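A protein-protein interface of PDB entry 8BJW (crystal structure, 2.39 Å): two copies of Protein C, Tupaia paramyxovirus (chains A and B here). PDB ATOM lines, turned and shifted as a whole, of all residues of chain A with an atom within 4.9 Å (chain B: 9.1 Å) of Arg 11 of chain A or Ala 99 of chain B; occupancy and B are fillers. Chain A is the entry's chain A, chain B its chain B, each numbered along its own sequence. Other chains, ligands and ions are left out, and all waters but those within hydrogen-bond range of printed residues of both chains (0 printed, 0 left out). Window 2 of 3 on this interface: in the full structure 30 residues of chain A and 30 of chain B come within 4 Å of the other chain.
Among the printed residues, merely in contact across the chains: Asn 12 of chain A with Met 95 of chain B (3.4 Å), Gln 13 of chain A with Glu 56 of chain B (3.4 Å), Asn 12 of chain A with Glu 56 of chain B (3.4 Å) and Leu 15 of chain A with Ala 98 of chain B (3.7 Å).
OE2 of Glu 56 of chain B sits at hydrogen-bond distance from ND1 of His 61 of chain B (2.6 Å).
ND2 of Asn 12 of chain A sits close to ND1 of His 61 of chain B, at 3.5 Å.
NE2 of Gln 13 of chain A is in hydrogen-bond range of O of Lys 57 of chain B, 3.3 Å away.
O of Ala 99 of chain B is in hydrogen-bond range of NH2 of Arg 11 of chain A, at 3.1 Å.
Of the 14 printed residues of chain B, 6 touch a printed residue of chain A.
Printed residues of chain B that touch a printed residue of chain A: Glu 56, Lys 57, His 61, Met 95, Ala 98 and Ala 99.
Hydrophobic or aromatic side chains of chain B within 4 Å of the printed part of chain A: His 61, Met 95, Ala 98 and Ala 99.
Among the printed residues, 7 pairs touch across the chains.
Of chain B, only Ala 99 (3.1 Å) comes within 4 Å of Arg 11 of chain A.
Of chain A, only Arg 11 comes within 4 Å of Ala 99 of chain B.
Of the printed residues of chain A, Met 95 of chain B touches Asn 12 (3.4 Å).
Of the printed residues of chain A, His 61 of chain B touches Asn 12.
Printed residues of chain A within 4 Å of Glu 56 of chain B: Asn 12 (3.4 Å) and Gln 13 (3.4 Å).
The nearest residue of chain A that does not touch Ala 99 of chain B is Leu 15 of chain A (4.1 Å).
The nearest printed residue of chain A that does not touch Ala 98 of chain B is Arg 11 of chain A (4.8 Å).
No position is printed for both chains.
Of the 7 pairs that touch across the chains among the printed residues, none has its exchanged pair printed and touching as well.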
ATOM      1  N   THR A   9      18.407  -8.401   3.726  1.00  0.00           N
ATOM      2  CA  THR A   9      19.687  -7.759   3.277  1.00  0.00           C
ATOM      3  C   THR A   9      19.975  -8.234   1.847  1.00  0.00           C
ATOM      4  O   THR A   9      19.658  -9.386   1.472  1.00  0.00           O
ATOM      5  CB  THR A   9      20.829  -7.939   4.308  1.00  0.00           C
ATOM      6  OG1 THR A   9      21.726  -6.809   4.347  1.00  0.00           O
ATOM      7  CG2 THR A   9      21.635  -9.224   4.172  1.00  0.00           C
ATOM      8  N   LYS A  10      20.536  -7.319   1.067  1.00  0.00           N
ATOM      9  CA  LYS A  10      20.962  -7.535  -0.338  1.00  0.00           C
ATOM     10  C   LYS A  10      22.098  -8.580  -0.372  1.00  0.00           C
ATOM     11  O   LYS A  10      22.267  -9.227  -1.412  1.00  0.00           O
ATOM     12  CB  LYS A  10      21.338  -6.172  -0.945  1.00  0.00           C
ATOM     13  CG  LYS A  10      21.372  -6.131  -2.464  1.00  0.00           C
ATOM     14  CD  LYS A  10      20.038  -6.457  -3.138  1.00  0.00           C
ATOM     15  CE  LYS A  10      20.157  -7.242  -4.437  1.00  0.00           C
ATOM     16  NZ  LYS A  10      21.344  -6.842  -5.228  1.00  0.00           N
ATOM     17  N   ARG A  11      22.843  -8.714   0.732  1.00  0.00           N
ATOM     18  CA  ARG A  11      23.983  -9.652   0.876  1.00  0.00           C
ATOM     19  C   ARG A  11      23.438 -11.078   0.728  1.00  0.00           C
ATOM     20  O   ARG A  11      23.966 -11.827  -0.109  1.00  0.00           O
ATOM     21  CB  ARG A  11      24.681  -9.456   2.229  1.00  0.00           C
ATOM     22  CG  ARG A  11      25.992 -10.215   2.330  1.00  0.00           C
ATOM     23  CD  ARG A  11      26.792 -10.029   3.614  1.00  0.00           C
ATOM     24  NE  ARG A  11      27.650 -11.195   3.840  1.00  0.00           N
ATOM     25  CZ  ARG A  11      28.932 -11.324   3.463  1.00  0.00           C
ATOM     26  NH1 ARG A  11      29.568 -10.335   2.856  1.00  0.00           N
ATOM     27  NH2 ARG A  11      29.574 -12.449   3.712  1.00  0.00           N
ATOM     28  N   ASN A  12      22.378 -11.400   1.476  1.00  0.00           N
ATOM     29  CA  ASN A  12      21.703 -12.716   1.436  1.00  0.00           C
ATOM     30  C   ASN A  12      21.301 -13.075   0.000  1.00  0.00           C
ATOM     31  O   ASN A  12      21.533 -14.234  -0.395  1.00  0.00           O
ATOM     32  CB  ASN A  12      20.538 -12.785   2.414  1.00  0.00           C
ATOM     33  CG  ASN A  12      20.985 -13.098   3.828  1.00  0.00           C
ATOM     34  OD1 ASN A  12      22.010 -13.744   4.047  1.00  0.00           O
ATOM     35  ND2 ASN A  12      20.178 -12.714   4.791  1.00  0.00           N
ATOM     36  N   GLN A  13      20.779 -12.115  -0.764  1.00  0.00           N
ATOM     37  CA  GLN A  13      20.267 -12.382  -2.136  1.00  0.00           C
ATOM     38  C   GLN A  13      21.413 -12.722  -3.082  1.00  0.00           C
ATOM     39  O   GLN A  13      21.272 -13.680  -3.880  1.00  0.00           O
ATOM     40  CB  GLN A  13      19.449 -11.208  -2.652  1.00  0.00           C
ATOM     41  CG  GLN A  13      18.144 -11.088  -1.889  1.00  0.00           C
ATOM     42  CD  GLN A  13      17.371  -9.857  -2.236  1.00  0.00           C
ATOM     43  OE1 GLN A  13      17.030  -9.090  -1.347  1.00  0.00           O
ATOM     44  NE2 GLN A  13      17.100  -9.680  -3.521  1.00  0.00           N
ATOM     45  N   GLU A  14      22.501 -11.971  -2.982  1.00  0.00           N
ATOM     46  CA  GLU A  14      23.712 -12.155  -3.824  1.00  0.00           C
ATOM     47  C   GLU A  14      24.368 -13.492  -3.458  1.00  0.00           C
ATOM     48  O   GLU A  14      24.762 -14.217  -4.379  1.00  0.00           O
ATOM     49  CB  GLU A  14      24.646 -10.940  -3.685  1.00  0.00           C
ATOM     50  CG  GLU A  14      23.996  -9.650  -4.199  1.00  0.00           C
ATOM     51  CD  GLU A  14      24.882  -8.497  -4.644  1.00  0.00           C
ATOM     52  OE1 GLU A  14      25.810  -8.721  -5.422  1.00  0.00           O
ATOM     53  OE2 GLU A  14      24.617  -7.383  -4.220  1.00  0.00           O
ATOM     54  N   LEU A  15      24.462 -13.821  -2.161  1.00  0.00           N
ATOM     55  CA  LEU A  15      24.992 -15.123  -1.689  1.00  0.00           C
ATOM     56  C   LEU A  15      24.207 -16.254  -2.368  1.00  0.00           C
ATOM     57  O   LEU A  15      24.849 -17.120  -2.999  1.00  0.00           O
ATOM     58  CB  LEU A  15      24.889 -15.196  -0.159  1.00  0.00           C
ATOM     59  CG  LEU A  15      25.896 -14.339   0.598  1.00  0.00           C
ATOM     60  CD1 LEU A  15      25.630 -14.397   2.092  1.00  0.00           C
ATOM     61  CD2 LEU A  15      27.312 -14.814   0.302  1.00  0.00           C
ATOM     62  N   GLU B  56      15.421 -17.361  -1.602  1.00  0.00           N
ATOM     63  CA  GLU B  56      16.427 -16.487  -0.958  1.00  0.00           C
ATOM     64  C   GLU B  56      16.910 -15.450  -1.976  1.00  0.00           C
ATOM     65  O   GLU B  56      16.953 -14.276  -1.648  1.00  0.00           O
ATOM     66  CB  GLU B  56      17.592 -17.328  -0.430  1.00  0.00           C
ATOM     67  CG  GLU B  56      18.541 -16.583   0.499  1.00  0.00           C
ATOM     68  CD  GLU B  56      18.007 -16.363   1.901  1.00  0.00           C
ATOM     69  OE1 GLU B  56      17.462 -17.344   2.460  1.00  0.00           O
ATOM     70  OE2 GLU B  56      18.094 -15.189   2.420  1.00  0.00           O
ATOM     71  N   LYS B  57      17.213 -15.870  -3.198  1.00  0.00           N
ATOM     72  CA  LYS B  57      17.734 -14.973  -4.251  1.00  0.00           C
ATOM     73  C   LYS B  57      16.693 -13.893  -4.518  1.00  0.00           C
ATOM     74  O   LYS B  57      17.100 -12.718  -4.691  1.00  0.00           O
ATOM     75  CB  LYS B  57      18.038 -15.733  -5.539  1.00  0.00           C
ATOM     76  CG  LYS B  57      18.433 -14.871  -6.728  1.00  0.00           C
ATOM     77  CD  LYS B  57      18.559 -15.660  -7.965  1.00  0.00           C
ATOM     78  CE  LYS B  57      18.876 -14.824  -9.174  1.00  0.00           C
ATOM     79  NZ  LYS B  57      19.271 -15.741 -10.262  1.00  0.00           N
ATOM     80  N   HIS B  61      13.685 -14.450   2.605  1.00  0.00           N
ATOM     81  CA  HIS B  61      14.737 -15.011   3.479  1.00  0.00           C
ATOM     82  C   HIS B  61      14.242 -16.369   3.983  1.00  0.00           C
ATOM     83  O   HIS B  61      13.076 -16.474   4.402  1.00  0.00           O
ATOM     84  CB  HIS B  61      15.123 -14.026   4.603  1.00  0.00           C
ATOM     85  CG  HIS B  61      16.248 -14.521   5.456  1.00  0.00           C
ATOM     86  ND1 HIS B  61      17.475 -14.915   4.921  1.00  0.00           N
ATOM     87  CD2 HIS B  61      16.333 -14.728   6.785  1.00  0.00           C
ATOM     88  CE1 HIS B  61      18.262 -15.340   5.895  1.00  0.00           C
ATOM     89  NE2 HIS B  61      17.577 -15.257   7.044  1.00  0.00           N
ATOM     90  N   VAL B  91      20.723 -25.638   3.074  1.00  0.00           N
ATOM     91  CA  VAL B  91      20.707 -24.224   2.594  1.00  0.00           C
ATOM     92  C   VAL B  91      21.405 -23.326   3.638  1.00  0.00           C
ATOM     93  O   VAL B  91      22.197 -22.451   3.259  1.00  0.00           O
ATOM     94  CB  VAL B  91      19.264 -23.767   2.300  1.00  0.00           C
ATOM     95  CG1 VAL B  91      19.122 -22.235   2.258  1.00  0.00           C
ATOM     96  CG2 VAL B  91      18.732 -24.383   1.018  1.00  0.00           C
ATOM     97  N   ARG B  92      21.090 -23.498   4.913  1.00  0.00           N
ATOM     98  CA  ARG B  92      21.700 -22.690   6.003  1.00  0.00           C
ATOM     99  C   ARG B  92      23.231 -22.888   5.987  1.00  0.00           C
ATOM    100  O   ARG B  92      23.970 -21.885   6.028  1.00  0.00           O
ATOM    101  CB  ARG B  92      21.086 -23.074   7.350  1.00  0.00           C
ATOM    102  CG  ARG B  92      19.604 -22.716   7.500  1.00  0.00           C
ATOM    103  CD  ARG B  92      19.274 -21.258   7.331  1.00  0.00           C
ATOM    104  NE  ARG B  92      19.839 -20.489   8.434  1.00  0.00           N
ATOM    105  CZ  ARG B  92      19.434 -19.257   8.812  1.00  0.00           C
ATOM    106  NH1 ARG B  92      18.471 -18.612   8.163  1.00  0.00           N
ATOM    107  NH2 ARG B  92      19.995 -18.682   9.861  1.00  0.00           N
ATOM    108  N   GLN B  93      23.697 -24.141   5.930  1.00  0.00           N
ATOM    109  CA  GLN B  93      25.143 -24.456   5.863  1.00  0.00           C
ATOM    110  C   GLN B  93      25.761 -23.704   4.671  1.00  0.00           C
ATOM    111  O   GLN B  93      26.794 -23.051   4.876  1.00  0.00           O
ATOM    112  CB  GLN B  93      25.404 -25.943   5.664  1.00  0.00           C
ATOM    113  CG  GLN B  93      25.324 -26.809   6.895  1.00  0.00           C
ATOM    114  CD  GLN B  93      25.574 -28.257   6.518  1.00  0.00           C
ATOM    115  OE1 GLN B  93      24.919 -29.151   7.050  1.00  0.00           O
ATOM    116  NE2 GLN B  93      26.496 -28.514   5.583  1.00  0.00           N
ATOM    117  N   MET B  94      25.133 -23.785   3.490  1.00  0.00           N
ATOM    118  CA  MET B  94      25.657 -23.199   2.235  1.00  0.00           C
ATOM    119  C   MET B  94      25.709 -21.688   2.382  1.00  0.00           C
ATOM    120  O   MET B  94      26.696 -21.107   1.880  1.00  0.00           O
ATOM    121  CB  MET B  94      24.808 -23.558   1.010  1.00  0.00           C
ATOM    122  CG  MET B  94      24.985 -25.021   0.560  1.00  0.00           C
ATOM    123  SD  MET B  94      23.795 -25.528  -0.750  1.00  0.00           S
ATOM    124  CE  MET B  94      24.253 -24.385  -2.044  1.00  0.00           C
ATOM    125  N   MET B  95      24.688 -21.058   2.982  1.00  0.00           N
ATOM    126  CA  MET B  95      24.668 -19.578   3.124  1.00  0.00           C
ATOM    127  C   MET B  95      25.816 -19.158   4.068  1.00  0.00           C
ATOM    128  O   MET B  95      26.479 -18.150   3.765  1.00  0.00           O
ATOM    129  CB  MET B  95      23.336 -19.061   3.677  1.00  0.00           C
ATOM    130  CG  MET B  95      22.185 -19.166   2.676  1.00  0.00           C
ATOM    131  SD  MET B  95      22.281 -18.026   1.296  1.00  0.00           S
ATOM    132  CE  MET B  95      21.830 -16.527   2.162  1.00  0.00           C
ATOM    133  N   HIS B  96      26.046 -19.923   5.141  1.00  0.00           N
ATOM    134  CA  HIS B  96      27.137 -19.683   6.123  1.00  0.00           C
ATOM    135  C   HIS B  96      28.507 -19.905   5.450  1.00  0.00           C
ATOM    136  O   HIS B  96      29.390 -19.030   5.568  1.00  0.00           O
ATOM    137  CB  HIS B  96      26.931 -20.515   7.404  1.00  0.00           C
ATOM    138  CG  HIS B  96      28.069 -20.384   8.361  1.00  0.00           C
ATOM    139  ND1 HIS B  96      29.087 -21.316   8.422  1.00  0.00           N
ATOM    140  CD2 HIS B  96      28.402 -19.419   9.251  1.00  0.00           C
ATOM    141  CE1 HIS B  96      29.985 -20.946   9.303  1.00  0.00           C
ATOM    142  NE2 HIS B  96      29.589 -19.798   9.836  1.00  0.00           N
ATOM    143  N   HIS B  97      28.675 -21.009   4.722  1.00  0.00           N
ATOM    144  CA  HIS B  97      29.916 -21.313   3.958  1.00  0.00           C
ATOM    145  C   HIS B  97      30.232 -20.192   2.958  1.00  0.00           C
ATOM    146  O   HIS B  97      31.394 -19.872   2.809  1.00  0.00           O
ATOM    147  CB  HIS B  97      29.814 -22.674   3.248  1.00  0.00           C
ATOM    148  CG  HIS B  97      31.014 -23.008   2.425  1.00  0.00           C
ATOM    149  ND1 HIS B  97      31.222 -22.445   1.182  1.00  0.00           N
ATOM    150  CD2 HIS B  97      32.021 -23.891   2.614  1.00  0.00           C
ATOM    151  CE1 HIS B  97      32.316 -22.954   0.646  1.00  0.00           C
ATOM    152  NE2 HIS B  97      32.818 -23.859   1.496  1.00  0.00           N
ATOM    153  N   ALA B  98      29.235 -19.639   2.267  1.00  0.00           N
ATOM    154  CA  ALA B  98      29.440 -18.583   1.246  1.00  0.00           C
ATOM    155  C   ALA B  98      29.845 -17.277   1.926  1.00  0.00           C
ATOM    156  O   ALA B  98      30.625 -16.525   1.329  1.00  0.00           O
ATOM    157  CB  ALA B  98      28.213 -18.389   0.399  1.00  0.00           C
ATOM    158  N   ALA B  99      29.341 -17.024   3.137  1.00  0.00           N
ATOM    159  CA  ALA B  99      29.614 -15.798   3.930  1.00  0.00           C
ATOM    160  C   ALA B  99      31.110 -15.744   4.293  1.00  0.00           C
ATOM    161  O   ALA B  99      31.691 -14.669   4.209  1.00  0.00           O
ATOM    162  CB  ALA B  99      28.739 -15.764   5.153  1.00  0.00           C
ATOM    163  N   LEU B 100      31.708 -16.871   4.714  1.00  0.00           N
ATOM    164  CA  LEU B 100      33.183 -17.076   4.737  1.00  0.00           C
ATOM    165  C   LEU B 100      33.528 -17.432   3.289  1.00  0.00           C
ATOM    166  O   LEU B 100      32.678 -18.070   2.648  1.00  0.00           O
ATOM    167  CB  LEU B 100      33.552 -18.216   5.701  1.00  0.00           C
ATOM    168  CG  LEU B 100      33.014 -18.122   7.133  1.00  0.00           C
ATOM    169  CD1 LEU B 100      33.406 -19.355   7.942  1.00  0.00           C
ATOM    170  CD2 LEU B 100      33.508 -16.847   7.803  1.00  0.00           C
ATOM    171  N   HIS B 101      34.679 -17.057   2.743  1.00  0.00           N
ATOM    172  CA  HIS B 101      35.062 -17.479   1.362  1.00  0.00           C
ATOM    173  C   HIS B 101      34.343 -16.563   0.365  1.00  0.00           C
ATOM    174  O   HIS B 101      33.456 -17.095  -0.310  1.00  0.00           O
ATOM    175  CB  HIS B 101      34.713 -18.966   1.075  1.00  0.00           C
ATOM    176  CG  HIS B 101      35.161 -19.932   2.126  1.00  0.00           C
ATOM    177  ND1 HIS B 101      36.476 -20.390   2.221  1.00  0.00           N
ATOM    178  CD2 HIS B 101      34.484 -20.511   3.141  1.00  0.00           C
ATOM    179  CE1 HIS B 101      36.571 -21.207   3.252  1.00  0.00           C
ATOM    180  NE2 HIS B 101      35.357 -21.293   3.838  1.00  0.00           N
